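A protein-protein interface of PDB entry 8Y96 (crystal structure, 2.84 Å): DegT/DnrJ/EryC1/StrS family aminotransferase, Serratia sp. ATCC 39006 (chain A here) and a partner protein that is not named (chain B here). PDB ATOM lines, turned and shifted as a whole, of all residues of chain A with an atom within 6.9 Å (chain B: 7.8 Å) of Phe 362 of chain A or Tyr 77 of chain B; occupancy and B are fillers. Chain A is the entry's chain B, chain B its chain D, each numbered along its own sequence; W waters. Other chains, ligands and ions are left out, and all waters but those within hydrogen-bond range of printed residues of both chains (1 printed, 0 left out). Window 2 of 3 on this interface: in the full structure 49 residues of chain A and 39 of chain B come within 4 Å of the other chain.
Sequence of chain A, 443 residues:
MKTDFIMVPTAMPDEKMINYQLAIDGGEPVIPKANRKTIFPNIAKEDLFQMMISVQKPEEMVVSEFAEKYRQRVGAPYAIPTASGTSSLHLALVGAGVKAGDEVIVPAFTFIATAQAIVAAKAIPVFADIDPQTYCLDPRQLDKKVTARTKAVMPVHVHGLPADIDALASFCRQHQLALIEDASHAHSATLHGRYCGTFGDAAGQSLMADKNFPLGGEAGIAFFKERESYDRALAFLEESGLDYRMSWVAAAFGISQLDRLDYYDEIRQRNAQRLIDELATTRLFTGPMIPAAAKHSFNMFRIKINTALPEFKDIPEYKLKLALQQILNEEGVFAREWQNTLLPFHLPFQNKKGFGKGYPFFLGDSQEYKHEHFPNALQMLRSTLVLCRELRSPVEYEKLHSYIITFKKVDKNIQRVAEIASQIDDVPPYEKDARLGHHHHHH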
ATOM      1  N   LYS A 122       6.801  19.908  34.913  1.00  0.00           N
ATOM      2  CA  LYS A 122       7.146  19.733  33.511  1.00  0.00           C
ATOM      3  C   LYS A 122       8.639  19.438  33.374  1.00  0.00           C
ATOM      4  O   LYS A 122       9.233  19.685  32.326  1.00  0.00           O
ATOM      5  CB  LYS A 122       6.626  20.938  32.714  1.00  0.00           C
ATOM      6  CG  LYS A 122       5.107  21.045  32.777  1.00  0.00           C
ATOM      7  CD  LYS A 122       4.462  22.207  32.035  1.00  0.00           C
ATOM      8  CE  LYS A 122       2.976  22.032  32.041  1.00  0.00           C
ATOM      9  NZ  LYS A 122       2.262  23.181  31.479  1.00  0.00           N
ATOM     10  N   ILE A 124      12.050  16.553  34.377  1.00  0.00           N
ATOM     11  CA  ILE A 124      12.369  15.155  34.151  1.00  0.00           C
ATOM     12  C   ILE A 124      13.113  14.615  35.370  1.00  0.00           C
ATOM     13  O   ILE A 124      14.240  15.015  35.642  1.00  0.00           O
ATOM     14  CB  ILE A 124      13.186  15.017  32.854  1.00  0.00           C
ATOM     15  CG1 ILE A 124      12.385  15.510  31.646  1.00  0.00           C
ATOM     16  CG2 ILE A 124      13.680  13.582  32.656  1.00  0.00           C
ATOM     17  CD1 ILE A 124      13.237  15.913  30.456  1.00  0.00           C
ATOM     18  N   LYS A 352       5.832   6.350  31.285  1.00  0.00           N
ATOM     19  CA  LYS A 352       6.339   7.685  30.990  1.00  0.00           C
ATOM     20  C   LYS A 352       5.301   8.476  30.196  1.00  0.00           C
ATOM     21  O   LYS A 352       5.623   9.091  29.185  1.00  0.00           O
ATOM     22  CB  LYS A 352       7.697   7.603  30.278  1.00  0.00           C
ATOM     23  CG  LYS A 352       8.835   7.110  31.160  1.00  0.00           C
ATOM     24  CD  LYS A 352      10.110   6.722  30.420  1.00  0.00           C
ATOM     25  CE  LYS A 352      11.203   6.340  31.370  1.00  0.00           C
ATOM     26  NZ  LYS A 352      12.442   5.978  30.677  1.00  0.00           N
ATOM     27  N   LYS A 353       4.057   8.469  30.686  1.00  0.00           N
ATOM     28  CA  LYS A 353       2.935   9.063  29.979  1.00  0.00           C
ATOM     29  C   LYS A 353       2.788  10.539  30.352  1.00  0.00           C
ATOM     30  O   LYS A 353       2.430  11.353  29.505  1.00  0.00           O
ATOM     31  CB  LYS A 353       1.678   8.236  30.272  1.00  0.00           C
ATOM     32  CG  LYS A 353       0.383   8.750  29.653  1.00  0.00           C
ATOM     33  CD  LYS A 353      -0.772   7.757  29.706  1.00  0.00           C
ATOM     34  CE  LYS A 353      -0.917   7.107  31.046  1.00  0.00           C
ATOM     35  NZ  LYS A 353      -2.178   6.373  31.152  1.00  0.00           N
ATOM     36  N   GLY A 354       3.042  10.879  31.622  1.00  0.00           N
ATOM     37  CA  GLY A 354       3.063  12.268  32.058  1.00  0.00           C
ATOM     38  C   GLY A 354       1.695  12.935  31.915  1.00  0.00           C
ATOM     39  O   GLY A 354       0.699  12.431  32.432  1.00  0.00           O
ATOM     40  N   PHE A 355       1.663  14.067  31.198  1.00  0.00           N
ATOM     41  CA  PHE A 355       0.436  14.811  30.956  1.00  0.00           C
ATOM     42  C   PHE A 355      -0.330  14.204  29.782  1.00  0.00           C
ATOM     43  O   PHE A 355      -1.378  14.725  29.402  1.00  0.00           O
ATOM     44  CB  PHE A 355       0.710  16.281  30.615  1.00  0.00           C
ATOM     45  CG  PHE A 355       1.194  17.173  31.751  1.00  0.00           C
ATOM     46  CD1 PHE A 355       2.535  17.205  32.120  1.00  0.00           C
ATOM     47  CD2 PHE A 355       0.310  18.016  32.421  1.00  0.00           C
ATOM     48  CE1 PHE A 355       2.970  18.036  33.140  1.00  0.00           C
ATOM     49  CE2 PHE A 355       0.752  18.845  33.441  1.00  0.00           C
ATOM     50  CZ  PHE A 355       2.078  18.854  33.799  1.00  0.00           C
ATOM     51  N   GLY A 356       0.201  13.111  29.216  1.00  0.00           N
ATOM     52  CA  GLY A 356      -0.282  12.559  27.961  1.00  0.00           C
ATOM     53  C   GLY A 356       0.796  12.666  26.885  1.00  0.00           C
ATOM     54  O   GLY A 356       1.532  13.649  26.845  1.00  0.00           O
ATOM     55  N   LYS A 357       0.893  11.627  26.042  1.00  0.00           N
ATOM     56  CA  LYS A 357       1.852  11.562  24.947  1.00  0.00           C
ATOM     57  C   LYS A 357       3.285  11.586  25.481  1.00  0.00           C
ATOM     58  O   LYS A 357       4.218  11.816  24.715  1.00  0.00           O
ATOM     59  CB  LYS A 357       1.690  12.726  23.960  1.00  0.00           C
ATOM     60  CG  LYS A 357       0.268  13.133  23.571  1.00  0.00           C
ATOM     61  CD  LYS A 357      -0.350  12.408  22.381  1.00  0.00           C
ATOM     62  CE  LYS A 357      -1.458  13.201  21.742  1.00  0.00           C
ATOM     63  NZ  LYS A 357      -2.648  13.351  22.587  1.00  0.00           N
ATOM     64  N   GLY A 358       3.455  11.347  26.789  1.00  0.00           N
ATOM     65  CA  GLY A 358       4.755  11.420  27.440  1.00  0.00           C
ATOM     66  C   GLY A 358       5.314  12.843  27.481  1.00  0.00           C
ATOM     67  O   GLY A 358       6.508  13.031  27.251  1.00  0.00           O
ATOM     68  N   TYR A 359       4.461  13.820  27.834  1.00  0.00           N
ATOM     69  CA  TYR A 359       4.760  15.225  27.594  1.00  0.00           C
ATOM     70  C   TYR A 359       6.122  15.570  28.189  1.00  0.00           C
ATOM     71  O   TYR A 359       7.050  15.872  27.441  1.00  0.00           O
ATOM     72  CB  TYR A 359       3.744  16.259  28.093  1.00  0.00           C
ATOM     73  CG  TYR A 359       4.322  17.668  28.178  1.00  0.00           C
ATOM     74  CD1 TYR A 359       5.161  18.167  27.186  1.00  0.00           C
ATOM     75  CD2 TYR A 359       4.072  18.484  29.274  1.00  0.00           C
ATOM     76  CE1 TYR A 359       5.711  19.436  27.271  1.00  0.00           C
ATOM     77  CE2 TYR A 359       4.615  19.754  29.370  1.00  0.00           C
ATOM     78  CZ  TYR A 359       5.437  20.234  28.367  1.00  0.00           C
ATOM     79  OH  TYR A 359       5.975  21.486  28.450  1.00  0.00           O
ATOM     80  N   PRO A 360       6.313  15.554  29.528  1.00  0.00           N
ATOM     81  CA  PRO A 360       7.556  16.073  30.101  1.00  0.00           C
ATOM     82  C   PRO A 360       8.770  15.327  29.549  1.00  0.00           C
ATOM     83  O   PRO A 360       9.771  15.942  29.188  1.00  0.00           O
ATOM     84  CB  PRO A 360       7.374  15.872  31.609  1.00  0.00           C
ATOM     85  CG  PRO A 360       5.880  15.724  31.779  1.00  0.00           C
ATOM     86  CD  PRO A 360       5.405  14.994  30.538  1.00  0.00           C
ATOM     87  N   PHE A 361       8.629  14.001  29.428  1.00  0.00           N
ATOM     88  CA  PHE A 361       9.755  13.097  29.261  1.00  0.00           C
ATOM     89  C   PHE A 361      10.407  13.244  27.887  1.00  0.00           C
ATOM     90  O   PHE A 361      11.619  13.074  27.774  1.00  0.00           O
ATOM     91  CB  PHE A 361       9.270  11.665  29.504  1.00  0.00           C
ATOM     92  CG  PHE A 361       8.771  11.424  30.922  1.00  0.00           C
ATOM     93  CD1 PHE A 361       9.667  11.230  31.970  1.00  0.00           C
ATOM     94  CD2 PHE A 361       7.409  11.393  31.205  1.00  0.00           C
ATOM     95  CE1 PHE A 361       9.211  11.012  33.261  1.00  0.00           C
ATOM     96  CE2 PHE A 361       6.959  11.175  32.499  1.00  0.00           C
ATOM     97  CZ  PHE A 361       7.860  10.986  33.523  1.00  0.00           C
ATOM     98  N   PHE A 362       9.620  13.563  26.850  1.00  0.00           N
ATOM     99  CA  PHE A 362      10.143  13.564  25.490  1.00  0.00           C
ATOM    100  C   PHE A 362      10.953  14.835  25.221  1.00  0.00           C
ATOM    101  O   PHE A 362      11.572  14.942  24.163  1.00  0.00           O
ATOM    102  CB  PHE A 362       9.024  13.288  24.478  1.00  0.00           C
ATOM    103  CG  PHE A 362       7.909  14.314  24.310  1.00  0.00           C
ATOM    104  CD1 PHE A 362       8.179  15.669  24.139  1.00  0.00           C
ATOM    105  CD2 PHE A 362       6.580  13.906  24.279  1.00  0.00           C
ATOM    106  CE1 PHE A 362       7.148  16.582  23.964  1.00  0.00           C
ATOM    107  CE2 PHE A 362       5.554  14.824  24.107  1.00  0.00           C
ATOM    108  CZ  PHE A 362       5.840  16.160  23.948  1.00  0.00           C
ATOM    109  N   LEU A 363      10.972  15.782  26.175  1.00  0.00           N
ATOM    110  CA  LEU A 363      11.806  16.973  26.062  1.00  0.00           C
ATOM    111  C   LEU A 363      13.285  16.604  26.163  1.00  0.00           C
ATOM    112  O   LEU A 363      14.126  17.317  25.619  1.00  0.00           O
ATOM    113  CB  LEU A 363      11.467  18.042  27.102  1.00  0.00           C
ATOM    114  CG  LEU A 363      10.268  18.961  26.829  1.00  0.00           C
ATOM    115  CD1 LEU A 363       9.764  18.910  25.394  1.00  0.00           C
ATOM    116  CD2 LEU A 363       9.126  18.707  27.801  1.00  0.00           C
ATOM    117  N   GLY A 364      13.598  15.513  26.876  1.00  0.00           N
ATOM    118  CA  GLY A 364      14.980  15.119  27.114  1.00  0.00           C
ATOM    119  C   GLY A 364      15.250  13.683  26.672  1.00  0.00           C
ATOM    120  O   GLY A 364      14.325  12.947  26.336  1.00  0.00           O
ATOM    121  N   ASP A 365      16.533  13.300  26.686  1.00  0.00           N
ATOM    122  CA  ASP A 365      16.950  11.962  26.299  1.00  0.00           C
ATOM    123  C   ASP A 365      16.408  10.948  27.303  1.00  0.00           C
ATOM    124  O   ASP A 365      16.515  11.156  28.506  1.00  0.00           O
ATOM    125  CB  ASP A 365      18.465  11.847  26.203  1.00  0.00           C
ATOM    126  CG  ASP A 365      19.129  12.688  25.124  1.00  0.00           C
ATOM    127  OD1 ASP A 365      18.405  13.383  24.378  1.00  0.00           O
ATOM    128  OD2 ASP A 365      20.372  12.639  25.037  1.00  0.00           O
ATOM    129  N   TRP B  71      -8.864  13.977  31.438  1.00  0.00           N
ATOM    130  CA  TRP B  71      -8.105  12.742  31.310  1.00  0.00           C
ATOM    131  C   TRP B  71      -9.042  11.538  31.370  1.00  0.00           C
ATOM    132  O   TRP B  71      -8.705  10.463  30.884  1.00  0.00           O
ATOM    133  CB  TRP B  71      -7.043  12.660  32.414  1.00  0.00           C
ATOM    134  CG  TRP B  71      -5.942  13.681  32.298  1.00  0.00           C
ATOM    135  CD1 TRP B  71      -5.819  14.688  31.384  1.00  0.00           C
ATOM    136  CD2 TRP B  71      -4.802  13.796  33.174  1.00  0.00           C
ATOM    137  NE1 TRP B  71      -4.675  15.405  31.614  1.00  0.00           N
ATOM    138  CE2 TRP B  71      -4.034  14.887  32.710  1.00  0.00           C
ATOM    139  CE3 TRP B  71      -4.362  13.084  34.296  1.00  0.00           C
ATOM    140  CZ2 TRP B  71      -2.850  15.277  33.333  1.00  0.00           C
ATOM    141  CZ3 TRP B  71      -3.193  13.472  34.910  1.00  0.00           C
ATOM    142  CH2 TRP B  71      -2.448  14.549  34.430  1.00  0.00           C
ATOM    143  N   ASP B  74      -9.652  10.837  27.833  1.00  0.00           N
ATOM    144  CA  ASP B  74      -8.445  10.887  27.022  1.00  0.00           C
ATOM    145  C   ASP B  74      -8.310  12.226  26.298  1.00  0.00           C
ATOM    146  O   ASP B  74      -7.786  12.274  25.187  1.00  0.00           O
ATOM    147  CB  ASP B  74      -8.376   9.696  26.082  1.00  0.00           C
ATOM    148  CG  ASP B  74      -8.518   8.352  26.779  1.00  0.00           C
ATOM    149  OD1 ASP B  74      -9.575   8.135  27.409  1.00  0.00           O
ATOM    150  OD2 ASP B  74      -7.563   7.551  26.713  1.00  0.00           O
ATOM    151  N   ILE B  75      -8.759  13.305  26.954  1.00  0.00           N
ATOM    152  CA  ILE B  75      -8.477  14.663  26.518  1.00  0.00           C
ATOM    153  C   ILE B  75      -7.264  15.153  27.309  1.00  0.00           C
ATOM    154  O   ILE B  75      -7.403  15.796  28.347  1.00  0.00           O
ATOM    155  CB  ILE B  75      -9.708  15.577  26.695  1.00  0.00           C
ATOM    156  CG1 ILE B  75     -10.979  14.941  26.113  1.00  0.00           C
ATOM    157  CG2 ILE B  75      -9.445  16.963  26.105  1.00  0.00           C
ATOM    158  CD1 ILE B  75     -12.254  15.719  26.393  1.00  0.00           C
ATOM    159  N   VAL B  76      -6.073  14.819  26.800  1.00  0.00           N
ATOM    160  CA  VAL B  76      -4.820  15.028  27.504  1.00  0.00           C
ATOM    161  C   VAL B  76      -3.959  15.998  26.697  1.00  0.00           C
ATOM    162  O   VAL B  76      -4.431  16.592  25.732  1.00  0.00           O
ATOM    163  CB  VAL B  76      -4.119  13.672  27.727  1.00  0.00           C
ATOM    164  CG1 VAL B  76      -5.033  12.668  28.422  1.00  0.00           C
ATOM    165  CG2 VAL B  76      -3.579  13.074  26.433  1.00  0.00           C
ATOM    166  N   TYR B  77      -2.697  16.160  27.112  1.00  0.00           N
ATOM    167  CA  TYR B  77      -1.774  17.067  26.447  1.00  0.00           C
ATOM    168  C   TYR B  77      -1.771  16.766  24.952  1.00  0.00           C
ATOM    169  O   TYR B  77      -1.581  15.621  24.552  1.00  0.00           O
ATOM    170  CB  TYR B  77      -0.379  16.935  27.066  1.00  0.00           C
ATOM    171  CG  TYR B  77       0.750  17.596  26.284  1.00  0.00           C
ATOM    172  CD1 TYR B  77       1.340  16.949  25.203  1.00  0.00           C
ATOM    173  CD2 TYR B  77       1.247  18.845  26.639  1.00  0.00           C
ATOM    174  CE1 TYR B  77       2.374  17.530  24.489  1.00  0.00           C
ATOM    175  CE2 TYR B  77       2.284  19.438  25.933  1.00  0.00           C
ATOM    176  CZ  TYR B  77       2.847  18.778  24.853  1.00  0.00           C
ATOM    177  OH  TYR B  77       3.872  19.329  24.139  1.00  0.00           O
ATOM    178  N   GLY B  78      -1.990  17.808  24.139  1.00  0.00           N
ATOM    179  CA  GLY B  78      -2.019  17.668  22.692  1.00  0.00           C
ATOM    180  C   GLY B  78      -3.446  17.609  22.147  1.00  0.00           C
ATOM    181  O   GLY B  78      -3.683  18.026  21.016  1.00  0.00           O
ATOM    182  N   GLU B  79      -4.387  17.093  22.952  1.00  0.00           N
ATOM    183  CA  GLU B  79      -5.774  16.949  22.531  1.00  0.00           C
ATOM    184  C   GLU B  79      -6.472  18.307  22.574  1.00  0.00           C
ATOM    185  O   GLU B  79      -5.830  19.335  22.788  1.00  0.00           O
ATOM    186  CB  GLU B  79      -6.492  15.899  23.385  1.00  0.00           C
ATOM    187  CG  GLU B  79      -5.915  14.493  23.228  1.00  0.00           C
ATOM    188  CD  GLU B  79      -5.982  13.920  21.822  1.00  0.00           C
ATOM    189  OE1 GLU B  79      -7.106  13.620  21.367  1.00  0.00           O
ATOM    190  OE2 GLU B  79      -4.916  13.783  21.179  1.00  0.00           O
ATOM    191  N   ALA B  80      -7.789  18.292  22.324  1.00  0.00           N
ATOM    192  CA  ALA B  80      -8.600  19.498  22.325  1.00  0.00           C
ATOM    193  C   ALA B  80     -10.036  19.156  22.706  1.00  0.00           C
ATOM    194  O   ALA B  80     -10.473  18.023  22.523  1.00  0.00           O
ATOM    195  CB  ALA B  80      -8.530  20.163  20.968  1.00  0.00           C
ATOM    196  N   PHE B  94      -6.642  24.524  31.456  1.00  0.00           N
ATOM    197  CA  PHE B  94      -6.569  23.784  30.206  1.00  0.00           C
ATOM    198  C   PHE B  94      -5.291  24.145  29.448  1.00  0.00           C
ATOM    199  O   PHE B  94      -4.640  23.276  28.874  1.00  0.00           O
ATOM    200  CB  PHE B  94      -7.781  24.073  29.315  1.00  0.00           C
ATOM    201  CG  PHE B  94      -9.105  23.440  29.727  1.00  0.00           C
ATOM    202  CD1 PHE B  94      -9.519  23.403  31.054  1.00  0.00           C
ATOM    203  CD2 PHE B  94      -9.942  22.879  28.768  1.00  0.00           C
ATOM    204  CE1 PHE B  94     -10.737  22.832  31.404  1.00  0.00           C
ATOM    205  CE2 PHE B  94     -11.153  22.304  29.123  1.00  0.00           C
ATOM    206  CZ  PHE B  94     -11.549  22.283  30.440  1.00  0.00           C
ATOM    207  N   LYS B  95      -4.935  25.432  29.439  1.00  0.00           N
ATOM    208  CA  LYS B  95      -3.717  25.883  28.781  1.00  0.00           C
ATOM    209  C   LYS B  95      -2.499  25.261  29.463  1.00  0.00           C
ATOM    210  O   LYS B  95      -1.503  24.980  28.801  1.00  0.00           O
ATOM    211  CB  LYS B  95      -3.665  27.415  28.778  1.00  0.00           C
ATOM    212  CG  LYS B  95      -2.565  28.064  27.949  1.00  0.00           C
ATOM    213  CD  LYS B  95      -2.821  29.554  27.729  1.00  0.00           C
ATOM    214  CE  LYS B  95      -1.868  30.221  26.787  1.00  0.00           C
ATOM    215  NZ  LYS B  95      -0.533  30.375  27.369  1.00  0.00           N
ATOM    216  N   TRP B  96      -2.588  25.046  30.784  1.00  0.00           N
ATOM    217  CA  TRP B  96      -1.511  24.418  31.536  1.00  0.00           C
ATOM    218  C   TRP B  96      -1.437  22.928  31.198  1.00  0.00           C
ATOM    219  O   TRP B  96      -0.347  22.386  31.029  1.00  0.00           O
ATOM    220  CB  TRP B  96      -1.676  24.650  33.048  1.00  0.00           C
ATOM    221  CG  TRP B  96      -0.569  24.023  33.857  1.00  0.00           C
ATOM    222  CD1 TRP B  96       0.721  24.457  33.961  1.00  0.00           C
ATOM    223  CD2 TRP B  96      -0.651  22.820  34.653  1.00  0.00           C
ATOM    224  NE1 TRP B  96       1.449  23.612  34.757  1.00  0.00           N
ATOM    225  CE2 TRP B  96       0.634  22.602  35.198  1.00  0.00           C
ATOM    226  CE3 TRP B  96      -1.674  21.915  34.955  1.00  0.00           C
ATOM    227  CZ2 TRP B  96       0.911  21.517  36.025  1.00  0.00           C
ATOM    228  CZ3 TRP B  96      -1.395  20.841  35.771  1.00  0.00           C
ATOM    229  CH2 TRP B  96      -0.119  20.647  36.298  1.00  0.00           C
ATOM    230  N   LEU B  97      -2.608  22.288  31.084  1.00  0.00           N
ATOM    231  CA  LEU B  97      -2.705  20.860  30.811  1.00  0.00           C
ATOM    232  C   LEU B  97      -2.274  20.528  29.381  1.00  0.00           C
ATOM    233  O   LEU B  97      -1.961  19.371  29.102  1.00  0.00           O
ATOM    234  CB  LEU B  97      -4.134  20.388  31.064  1.00  0.00           C
ATOM    235  CG  LEU B  97      -4.522  20.163  32.525  1.00  0.00           C
ATOM    236  CD1 LEU B  97      -6.025  20.007  32.635  1.00  0.00           C
ATOM    237  CD2 LEU B  97      -3.815  18.946  33.103  1.00  0.00           C
ATOM    238  N   GLY B  98      -2.310  21.525  28.481  1.00  0.00           N
ATOM    239  CA  GLY B  98      -1.872  21.361  27.101  1.00  0.00           C
ATOM    240  C   GLY B  98      -3.035  21.254  26.109  1.00  0.00           C
ATOM    241  O   GLY B  98      -2.800  21.202  24.904  1.00  0.00           O
ATOM    242  N   ILE B  99      -4.278  21.232  26.615  1.00  0.00           N
ATOM    243  CA  ILE B  99      -5.469  21.081  25.790  1.00  0.00           C
ATOM    244  C   ILE B  99      -5.775  22.393  25.059  1.00  0.00           C
ATOM    245  O   ILE B  99      -5.580  23.478  25.609  1.00  0.00           O
ATOM    246  CB  ILE B  99      -6.663  20.618  26.648  1.00  0.00           C
ATOM    247  CG1 ILE B  99      -6.517  19.160  27.102  1.00  0.00           C
ATOM    248  CG2 ILE B  99      -7.992  20.831  25.925  1.00  0.00           C
ATOM    249  CD1 ILE B  99      -5.776  18.977  28.412  1.00  0.00           C
ATOM    250  N   GLY B 100      -6.279  22.274  23.818  1.00  0.00           N
ATOM    251  CA  GLY B 100      -6.699  23.407  23.004  1.00  0.00           C
ATOM    252  C   GLY B 100      -8.215  23.425  22.787  1.00  0.00           C
ATOM    253  O   GLY B 100      -8.939  22.600  23.348  1.00  0.00           O
HETATM  254  O   HOH W   1      -2.831  17.086  30.193  1.00  0.00           O
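The side-chain amino group (NZ) of Lys 122 of chain A lies within hydrogen-bond range of the backbone carbonyl oxygen (O) of Trp 96 of chain B. N of Tyr 77 of chain B sits at hydrogen-bond distance from O of Phe 355 of chain A (3.0 Å). The side-chain amino group of Lys 357 of chain A lies within hydrogen-bond range of the backbone carbonyl oxygen of Tyr 77 of chain B (3.2 Å). The side-chain amino group of Lys 357 of chain A lies within salt-bridge range of the side-chain carboxylate of Glu 79 of chain B (2.7 Å).
The backbone carbonyl oxygen of Glu 79 of chain B is in hydrogen-bond range of the backbone NH of Gly 100 of chain B, at 3.1 Å.
CB of Val 76 of chain B touches O of Phe 355 of chain A, 3.4 Å away. CE2 of Phe 355 of chain A touches CH2 of Trp 96 of chain B, at 3.5 Å. CA of Gly 356 of chain A touches CG2 of Val 76 of chain B (3.7 Å). Tyr 77 of chain B touches Gly 356 of chain A. NZ of Lys 357 of chain A touches CG2 of Val 76 of chain B, 3.97 Å away. CD1 of Tyr 359 of chain A touches CZ of Tyr 77 of chain B, 3.3 Å away. Phe 362 of chain A touches Tyr 77 of chain B (CZ to OH, 3.7 Å).
Tyr 77 of chain B touches five residues of chain A. Of the printed residues of chain B, Lys 122 of chain A touches Trp 96. Of the printed residues of chain B, Phe 355 of chain A touches Val 76, Tyr 77 and Trp 96. Leu 363 of chain A touches none of the printed residues of chain B. The nearest printed residue of chain B that does not touch Phe 362 of chain A is Gly 78 of chain B (8.0 Å). The nearest printed residue of chain B that does not touch Phe 355 of chain A is Trp 71 of chain B (4.03 Å).
Of the 16 printed residues of chain A, 6 touch a printed residue of chain B. Printed residues of chain A that touch a printed residue of chain B: Lys 122, Phe 355, Gly 356, Lys 357, Tyr 359 and Phe 362. Hydrophobic or aromatic side chains of chain A that line the printed part of chain B: Phe 355, Tyr 359 and Phe 362. Of the 15 printed residues of chain B, 4 touch a printed residue of chain A. Printed residues of chain B that touch a printed residue of chain A: Val 76, Tyr 77, Glu 79 and Trp 96. Hydrophobic or aromatic side chains of chain B that line the printed part of chain A: Val 76, Tyr 77 and Trp 96. Along chain B the printed residues that touch a printed residue of chain A span positions 76 to 96. Among the printed residues, 11 pairs touch across the chains. Among the printed residues, Asp or Glu carboxylates within 4 Å of a Lys or Arg side-chain nitrogen of the other chain: Lys 357 of chain A with Glu 79 of chain B (2.7 Å).
Water W1 lies within hydrogen-bond range of the backbone carbonyl oxygen of Leu 97 of chain B (2.7 Å), the indole nitrogen of Trp 71 of chain B (2.9 Å), the backbone carbonyl oxygen of Phe 355 of chain A (2.9 Å) and the backbone NH of Tyr 77 of chain B (3.2 Å).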
